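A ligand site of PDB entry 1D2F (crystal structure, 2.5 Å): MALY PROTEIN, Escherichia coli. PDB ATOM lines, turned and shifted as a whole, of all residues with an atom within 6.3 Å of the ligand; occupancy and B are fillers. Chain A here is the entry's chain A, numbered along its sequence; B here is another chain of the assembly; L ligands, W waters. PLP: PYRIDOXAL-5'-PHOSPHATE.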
ATOM      1  N   SER A  36     -19.531 -24.567  -6.688  1.00  0.00           N
ATOM      2  CA  SER A  36     -18.557 -23.848  -5.883  1.00  0.00           C
ATOM      3  C   SER A  36     -17.087 -24.257  -5.903  1.00  0.00           C
ATOM      4  O   SER A  36     -16.220 -23.411  -5.656  1.00  0.00           O
ATOM      5  CB  SER A  36     -19.056 -23.851  -4.438  1.00  0.00           C
ATOM      6  OG  SER A  36     -20.466 -23.644  -4.382  1.00  0.00           O
ATOM      7  N   PRO A  94     -15.801 -27.446  12.068  1.00  0.00           N
ATOM      8  CA  PRO A  94     -15.988 -28.508  11.066  1.00  0.00           C
ATOM      9  C   PRO A  94     -16.121 -27.891   9.672  1.00  0.00           C
ATOM     10  O   PRO A  94     -15.671 -28.456   8.691  1.00  0.00           O
ATOM     11  CB  PRO A  94     -17.287 -29.185  11.488  1.00  0.00           C
ATOM     12  CG  PRO A  94     -17.418 -28.867  12.945  1.00  0.00           C
ATOM     13  CD  PRO A  94     -16.918 -27.444  13.029  1.00  0.00           C
ATOM     14  N   SER A  95     -16.774 -26.734   9.626  1.00  0.00           N
ATOM     15  CA  SER A  95     -16.980 -26.015   8.388  1.00  0.00           C
ATOM     16  C   SER A  95     -17.234 -24.552   8.728  1.00  0.00           C
ATOM     17  O   SER A  95     -17.526 -24.221   9.878  1.00  0.00           O
ATOM     18  CB  SER A  95     -18.185 -26.570   7.650  1.00  0.00           C
ATOM     19  OG  SER A  95     -19.363 -26.256   8.350  1.00  0.00           O
ATOM     20  N   VAL A  96     -17.131 -23.677   7.738  1.00  0.00           N
ATOM     21  CA  VAL A  96     -17.376 -22.264   7.988  1.00  0.00           C
ATOM     22  C   VAL A  96     -18.816 -22.009   8.376  1.00  0.00           C
ATOM     23  O   VAL A  96     -19.095 -21.302   9.337  1.00  0.00           O
ATOM     24  CB  VAL A  96     -17.015 -21.404   6.766  1.00  0.00           C
ATOM     25  CG1 VAL A  96     -17.551 -19.987   6.937  1.00  0.00           C
ATOM     26  CG2 VAL A  96     -15.505 -21.378   6.600  1.00  0.00           C
ATOM     27  N   ILE A  97     -19.755 -22.593   7.631  1.00  0.00           N
ATOM     28  CA  ILE A  97     -21.164 -22.397   7.911  1.00  0.00           C
ATOM     29  C   ILE A  97     -21.560 -22.871   9.311  1.00  0.00           C
ATOM     30  O   ILE A  97     -22.445 -22.290   9.937  1.00  0.00           O
ATOM     31  CB  ILE A  97     -22.030 -23.110   6.860  1.00  0.00           C
ATOM     32  CG1 ILE A  97     -21.665 -22.591   5.456  1.00  0.00           C
ATOM     33  CG2 ILE A  97     -23.506 -22.870   7.137  1.00  0.00           C
ATOM     34  CD1 ILE A  97     -21.879 -21.101   5.268  1.00  0.00           C
ATOM     35  N   TYR A  98     -20.911 -23.916   9.815  1.00  0.00           N
ATOM     36  CA  TYR A  98     -21.231 -24.400  11.154  1.00  0.00           C
ATOM     37  C   TYR A  98     -20.893 -23.307  12.142  1.00  0.00           C
ATOM     38  O   TYR A  98     -21.614 -23.077  13.114  1.00  0.00           O
ATOM     39  CB  TYR A  98     -20.435 -25.656  11.514  1.00  0.00           C
ATOM     40  CG  TYR A  98     -20.615 -26.030  12.971  1.00  0.00           C
ATOM     41  CD1 TYR A  98     -21.774 -26.641  13.420  1.00  0.00           C
ATOM     42  CD2 TYR A  98     -19.659 -25.651  13.911  1.00  0.00           C
ATOM     43  CE1 TYR A  98     -21.988 -26.865  14.776  1.00  0.00           C
ATOM     44  CE2 TYR A  98     -19.865 -25.878  15.277  1.00  0.00           C
ATOM     45  CZ  TYR A  98     -21.021 -26.474  15.701  1.00  0.00           C
ATOM     46  OH  TYR A  98     -21.240 -26.610  17.048  1.00  0.00           O
ATOM     47  N   TYR A 121     -24.619 -15.737  -0.914  1.00  0.00           N
ATOM     48  CA  TYR A 121     -24.322 -17.154  -1.007  1.00  0.00           C
ATOM     49  C   TYR A 121     -25.513 -17.886  -0.390  1.00  0.00           C
ATOM     50  O   TYR A 121     -25.892 -17.624   0.754  1.00  0.00           O
ATOM     51  CB  TYR A 121     -23.039 -17.435  -0.222  1.00  0.00           C
ATOM     52  CG  TYR A 121     -22.645 -18.889  -0.125  1.00  0.00           C
ATOM     53  CD1 TYR A 121     -22.461 -19.672  -1.270  1.00  0.00           C
ATOM     54  CD2 TYR A 121     -22.389 -19.466   1.117  1.00  0.00           C
ATOM     55  CE1 TYR A 121     -22.031 -20.989  -1.177  1.00  0.00           C
ATOM     56  CE2 TYR A 121     -21.950 -20.784   1.221  1.00  0.00           C
ATOM     57  CZ  TYR A 121     -21.773 -21.538   0.077  1.00  0.00           C
ATOM     58  OH  TYR A 121     -21.331 -22.829   0.193  1.00  0.00           O
ATOM     59  N   PHE A 124     -26.221 -18.890   3.387  1.00  0.00           N
ATOM     60  CA  PHE A 124     -26.512 -17.888   4.419  1.00  0.00           C
ATOM     61  C   PHE A 124     -27.986 -17.885   4.807  1.00  0.00           C
ATOM     62  O   PHE A 124     -28.331 -17.733   5.986  1.00  0.00           O
ATOM     63  CB  PHE A 124     -26.115 -16.488   3.954  1.00  0.00           C
ATOM     64  CG  PHE A 124     -24.632 -16.263   3.880  1.00  0.00           C
ATOM     65  CD1 PHE A 124     -24.121 -15.079   3.369  1.00  0.00           C
ATOM     66  CD2 PHE A 124     -23.735 -17.231   4.321  1.00  0.00           C
ATOM     67  CE1 PHE A 124     -22.751 -14.868   3.291  1.00  0.00           C
ATOM     68  CE2 PHE A 124     -22.370 -17.024   4.256  1.00  0.00           C
ATOM     69  CZ  PHE A 124     -21.869 -15.839   3.734  1.00  0.00           C
ATOM     70  N   CYS A 169     -19.721 -11.067   3.910  1.00  0.00           N
ATOM     71  CA  CYS A 169     -18.988 -11.941   3.016  1.00  0.00           C
ATOM     72  C   CYS A 169     -17.895 -11.059   2.394  1.00  0.00           C
ATOM     73  O   CYS A 169     -18.187 -10.205   1.556  1.00  0.00           O
ATOM     74  CB  CYS A 169     -19.906 -12.497   1.924  1.00  0.00           C
ATOM     75  SG  CYS A 169     -19.138 -13.808   0.954  1.00  0.00           S
ATOM     76  N   PRO A 171     -13.935 -11.444   0.700  1.00  0.00           N
ATOM     77  CA  PRO A 171     -14.571 -10.897  -0.492  1.00  0.00           C
ATOM     78  C   PRO A 171     -16.006 -11.371  -0.610  1.00  0.00           C
ATOM     79  O   PRO A 171     -16.371 -12.403  -0.068  1.00  0.00           O
ATOM     80  CB  PRO A 171     -13.687 -11.416  -1.624  1.00  0.00           C
ATOM     81  CG  PRO A 171     -12.351 -11.501  -1.001  1.00  0.00           C
ATOM     82  CD  PRO A 171     -12.691 -12.136   0.336  1.00  0.00           C
ATOM     83  N   ASN A 173     -19.286 -12.901  -2.404  1.00  0.00           N
ATOM     84  CA  ASN A 173     -19.645 -13.924  -3.373  1.00  0.00           C
ATOM     85  C   ASN A 173     -21.140 -13.719  -3.632  1.00  0.00           C
ATOM     86  O   ASN A 173     -21.938 -13.626  -2.697  1.00  0.00           O
ATOM     87  CB  ASN A 173     -19.380 -15.297  -2.751  1.00  0.00           C
ATOM     88  CG  ASN A 173     -19.955 -16.438  -3.571  1.00  0.00           C
ATOM     89  OD1 ASN A 173     -20.367 -16.247  -4.712  1.00  0.00           O
ATOM     90  ND2 ASN A 173     -19.958 -17.624  -2.996  1.00  0.00           N
ATOM     91  N   ASP A 201     -17.078 -13.647   6.836  1.00  0.00           N
ATOM     92  CA  ASP A 201     -16.783 -14.879   6.123  1.00  0.00           C
ATOM     93  C   ASP A 201     -15.765 -14.490   5.055  1.00  0.00           C
ATOM     94  O   ASP A 201     -16.111 -13.898   4.042  1.00  0.00           O
ATOM     95  CB  ASP A 201     -18.069 -15.420   5.487  1.00  0.00           C
ATOM     96  CG  ASP A 201     -17.856 -16.683   4.670  1.00  0.00           C
ATOM     97  OD1 ASP A 201     -18.870 -17.262   4.231  1.00  0.00           O
ATOM     98  OD2 ASP A 201     -16.694 -17.090   4.466  1.00  0.00           O
ATOM     99  N   ILE A 203     -13.596 -16.673   3.356  1.00  0.00           N
ATOM    100  CA  ILE A 203     -13.086 -17.866   2.699  1.00  0.00           C
ATOM    101  C   ILE A 203     -12.538 -17.636   1.282  1.00  0.00           C
ATOM    102  O   ILE A 203     -11.857 -18.496   0.722  1.00  0.00           O
ATOM    103  CB  ILE A 203     -14.184 -18.968   2.679  1.00  0.00           C
ATOM    104  CG1 ILE A 203     -13.582 -20.298   2.235  1.00  0.00           C
ATOM    105  CG2 ILE A 203     -15.318 -18.550   1.782  1.00  0.00           C
ATOM    106  CD1 ILE A 203     -14.411 -21.497   2.631  1.00  0.00           C
ATOM    107  N   HIS A 204     -12.801 -16.464   0.696  1.00  0.00           N
ATOM    108  CA  HIS A 204     -12.271 -16.178  -0.633  1.00  0.00           C
ATOM    109  C   HIS A 204     -11.077 -15.241  -0.580  1.00  0.00           C
ATOM    110  O   HIS A 204     -10.564 -14.817  -1.618  1.00  0.00           O
ATOM    111  CB  HIS A 204     -13.336 -15.572  -1.541  1.00  0.00           C
ATOM    112  CG  HIS A 204     -14.324 -16.573  -2.030  1.00  0.00           C
ATOM    113  ND1 HIS A 204     -15.508 -16.831  -1.371  1.00  0.00           N
ATOM    114  CD2 HIS A 204     -14.280 -17.438  -3.070  1.00  0.00           C
ATOM    115  CE1 HIS A 204     -16.142 -17.809  -1.980  1.00  0.00           C
ATOM    116  NE2 HIS A 204     -15.421 -18.198  -3.015  1.00  0.00           N
ATOM    117  N   SER A 230     -10.837 -20.772   5.805  1.00  0.00           N
ATOM    118  CA  SER A 230     -10.370 -22.123   5.582  1.00  0.00           C
ATOM    119  C   SER A 230      -9.555 -22.078   4.285  1.00  0.00           C
ATOM    120  O   SER A 230      -9.582 -21.092   3.545  1.00  0.00           O
ATOM    121  CB  SER A 230     -11.559 -23.066   5.415  1.00  0.00           C
ATOM    122  OG  SER A 230     -11.226 -24.168   4.606  1.00  0.00           O
ATOM    123  N   SER A 232      -9.982 -24.439   2.108  1.00  0.00           N
ATOM    124  CA  SER A 232     -10.752 -25.294   1.228  1.00  0.00           C
ATOM    125  C   SER A 232     -11.078 -24.712  -0.130  1.00  0.00           C
ATOM    126  O   SER A 232     -11.074 -25.434  -1.122  1.00  0.00           O
ATOM    127  CB  SER A 232     -12.057 -25.766   1.908  1.00  0.00           C
ATOM    128  OG  SER A 232     -12.951 -24.694   2.128  1.00  0.00           O
ATOM    129  N   LYS A 233     -11.354 -23.422  -0.185  1.00  0.00           N
ATOM    130  CA  LYS A 233     -11.672 -22.803  -1.461  1.00  0.00           C
ATOM    131  C   LYS A 233     -10.407 -22.517  -2.278  1.00  0.00           C
ATOM    132  O   LYS A 233     -10.389 -22.712  -3.490  1.00  0.00           O
ATOM    133  CB  LYS A 233     -12.473 -21.518  -1.240  1.00  0.00           C
ATOM    134  CG  LYS A 233     -13.765 -21.455  -2.057  1.00  0.00           C
ATOM    135  CD  LYS A 233     -14.521 -22.781  -2.031  1.00  0.00           C
ATOM    136  CE  LYS A 233     -15.997 -22.610  -2.384  1.00  0.00           C
ATOM    137  NZ  LYS A 233     -16.608 -21.798  -1.325  1.00  0.00           N
ATOM    138  N   PRO A 238     -12.110 -29.080  -0.032  1.00  0.00           N
ATOM    139  CA  PRO A 238     -13.276 -29.123   0.850  1.00  0.00           C
ATOM    140  C   PRO A 238     -13.629 -30.546   1.333  1.00  0.00           C
ATOM    141  O   PRO A 238     -14.151 -30.725   2.447  1.00  0.00           O
ATOM    142  CB  PRO A 238     -14.382 -28.516  -0.025  1.00  0.00           C
ATOM    143  CG  PRO A 238     -14.003 -28.942  -1.388  1.00  0.00           C
ATOM    144  CD  PRO A 238     -12.502 -28.668  -1.395  1.00  0.00           C
ATOM    145  N   GLY A 242     -12.965 -29.132   7.680  1.00  0.00           N
ATOM    146  CA  GLY A 242     -12.114 -28.285   8.476  1.00  0.00           C
ATOM    147  C   GLY A 242     -12.216 -26.833   8.067  1.00  0.00           C
ATOM    148  O   GLY A 242     -12.438 -26.493   6.893  1.00  0.00           O
ATOM    149  N   ALA A 243     -12.048 -25.965   9.050  1.00  0.00           N
ATOM    150  CA  ALA A 243     -12.098 -24.539   8.849  1.00  0.00           C
ATOM    151  C   ALA A 243     -11.545 -24.014  10.160  1.00  0.00           C
ATOM    152  O   ALA A 243     -11.338 -24.799  11.103  1.00  0.00           O
ATOM    153  CB  ALA A 243     -13.536 -24.072   8.628  1.00  0.00           C
ATOM    154  N   LEU A 323     -15.263 -17.142  -9.929  1.00  0.00           N
ATOM    155  CA  LEU A 323     -16.643 -17.252 -10.370  1.00  0.00           C
ATOM    156  C   LEU A 323     -16.945 -15.993 -11.174  1.00  0.00           C
ATOM    157  O   LEU A 323     -16.566 -14.895 -10.778  1.00  0.00           O
ATOM    158  CB  LEU A 323     -17.595 -17.318  -9.179  1.00  0.00           C
ATOM    159  CG  LEU A 323     -17.527 -18.513  -8.243  1.00  0.00           C
ATOM    160  CD1 LEU A 323     -18.335 -18.204  -6.991  1.00  0.00           C
ATOM    161  CD2 LEU A 323     -18.061 -19.765  -8.943  1.00  0.00           C
ATOM    162  N   TYR B  61     -15.898 -31.274  -3.523  1.00  0.00           N
ATOM    163  CA  TYR B  61     -17.085 -31.733  -2.797  1.00  0.00           C
ATOM    164  C   TYR B  61     -17.530 -33.141  -3.204  1.00  0.00           C
ATOM    165  O   TYR B  61     -17.602 -33.479  -4.386  1.00  0.00           O
ATOM    166  CB  TYR B  61     -18.233 -30.739  -3.000  1.00  0.00           C
ATOM    167  CG  TYR B  61     -18.056 -29.409  -2.287  1.00  0.00           C
ATOM    168  CD1 TYR B  61     -17.933 -29.356  -0.894  1.00  0.00           C
ATOM    169  CD2 TYR B  61     -18.026 -28.200  -2.997  1.00  0.00           C
ATOM    170  CE1 TYR B  61     -17.786 -28.147  -0.226  1.00  0.00           C
ATOM    171  CE2 TYR B  61     -17.882 -26.977  -2.333  1.00  0.00           C
ATOM    172  CZ  TYR B  61     -17.759 -26.965  -0.947  1.00  0.00           C
ATOM    173  OH  TYR B  61     -17.616 -25.764  -0.276  1.00  0.00           O
ATOM    174  N   GLY B 265     -24.738 -26.554   8.139  1.00  0.00           N
ATOM    175  CA  GLY B 265     -23.771 -26.685   7.055  1.00  0.00           C
ATOM    176  C   GLY B 265     -22.713 -27.779   7.230  1.00  0.00           C
ATOM    177  O   GLY B 265     -21.516 -27.515   7.043  1.00  0.00           O
ATOM    178  N   LEU B 266     -23.139 -29.000   7.541  1.00  0.00           N
ATOM    179  CA  LEU B 266     -22.224 -30.125   7.749  1.00  0.00           C
ATOM    180  C   LEU B 266     -22.511 -31.319   6.857  1.00  0.00           C
ATOM    181  O   LEU B 266     -22.058 -32.419   7.151  1.00  0.00           O
ATOM    182  CB  LEU B 266     -22.290 -30.604   9.197  1.00  0.00           C
ATOM    183  CG  LEU B 266     -21.927 -29.660  10.340  1.00  0.00           C
ATOM    184  CD1 LEU B 266     -22.495 -30.194  11.637  1.00  0.00           C
ATOM    185  CD2 LEU B 266     -20.421 -29.510  10.417  1.00  0.00           C
ATOM    186  N   SER B 268     -21.461 -31.931   3.834  1.00  0.00           N
ATOM    187  CA  SER B 268     -20.274 -32.344   3.082  1.00  0.00           C
ATOM    188  C   SER B 268     -19.379 -33.170   4.004  1.00  0.00           C
ATOM    189  O   SER B 268     -18.818 -32.656   4.970  1.00  0.00           O
ATOM    190  CB  SER B 268     -19.529 -31.102   2.579  1.00  0.00           C
ATOM    191  OG  SER B 268     -18.277 -31.463   2.030  1.00  0.00           O
HETATM  192  N1  PLP L   1     -18.737 -19.144   2.378  1.00  0.00           N
HETATM  193  C2  PLP L   1     -18.728 -18.765   1.039  1.00  0.00           C
HETATM  194  C2A PLP L   1     -19.111 -17.316   0.806  1.00  0.00           C
HETATM  195  C3  PLP L   1     -18.348 -19.822   0.055  1.00  0.00           C
HETATM  196  O3  PLP L   1     -18.399 -19.404  -1.212  1.00  0.00           O
HETATM  197  C4  PLP L   1     -18.012 -21.094   0.494  1.00  0.00           C
HETATM  198  C4A PLP L   1     -17.617 -22.124  -0.489  1.00  0.00           C
HETATM  199  C5  PLP L   1     -18.053 -21.364   1.977  1.00  0.00           C
HETATM  200  C6  PLP L   1     -18.428 -20.368   2.865  1.00  0.00           C
HETATM  201  C5A PLP L   1     -17.614 -22.715   2.492  1.00  0.00           C
HETATM  202  O4P PLP L   1     -18.567 -23.346   3.313  1.00  0.00           O
HETATM  203  P   PLP L   1     -18.212 -24.810   3.921  1.00  0.00           P
HETATM  204  O1P PLP L   1     -19.388 -24.999   4.831  1.00  0.00           O
HETATM  205  O2P PLP L   1     -16.885 -24.651   4.758  1.00  0.00           O
HETATM  206  O3P PLP L   1     -18.048 -25.626   2.640  1.00  0.00           O
HETATM  207  O   HOH W   1     -20.016 -25.334   1.297  1.00  0.00           O
HETATM  208  O   HOH W   2     -18.433 -28.477   3.631  1.00  0.00           O
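A carbon (C4A) of the ligand is covalently linked to the side-chain amino group (NZ) of Lys 233, 1.4 Å away. The side-chain carboxylate (OD1) of Asp 201 is in hydrogen-bond range of a nitrogen (N1) of the ligand. An oxygen (O3P) of the ligand is in hydrogen-bond range of the side-chain hydroxyl (OH) of Tyr 61 of chain B, 3.0 Å away. O3 of the ligand lies within hydrogen-bond range of ND2 of Asn 173. The backbone NH (N) of Val 96 is in hydrogen-bond range of an oxygen (O2P) of the ligand, at 3.1 Å.
The side-chain carboxylate (OD2) of Asp 201 sits at hydrogen-bond distance from the backbone NH (N) of Ile 203 (3.3 Å). The side-chain sulfur of Cys 169 sits at hydrogen-bond distance from the backbone NH of Asn 173. OG of Ser 95 is in hydrogen-bond range of O of Gly 265 of chain B, at 2.8 Å. OG of Ser 95 is in hydrogen-bond range of N of Tyr 98, at 3.2 Å. The backbone carbonyl oxygen of Pro 171 lies close to the side-chain sulfur of Cys 169 (3.3 Å).
Residues that only touch the ligand: Ser 95 (3.4 Å), Ile 97 (3.4 Å), Tyr 121 (3.7 Å), Cys 169 (3.5 Å), Ile 203 (3.4 Å), His 204 (2.9 Å) and Gly 265 of chain B (3.97 Å). Of the 25 residues printed, 12 come within 4 Å of the ligand.
Water W1 lies within hydrogen-bond range of an oxygen (O3P) of the ligand (2.4 Å), the side-chain hydroxyl (OH) of Tyr 61 of chain B (2.9 Å) and the side-chain hydroxyl (OH) of Tyr 121 (3.0 Å). Water W2 bridges O3P of the ligand (3.0 Å) and OG of Ser 268 of chain B (3.4 Å).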
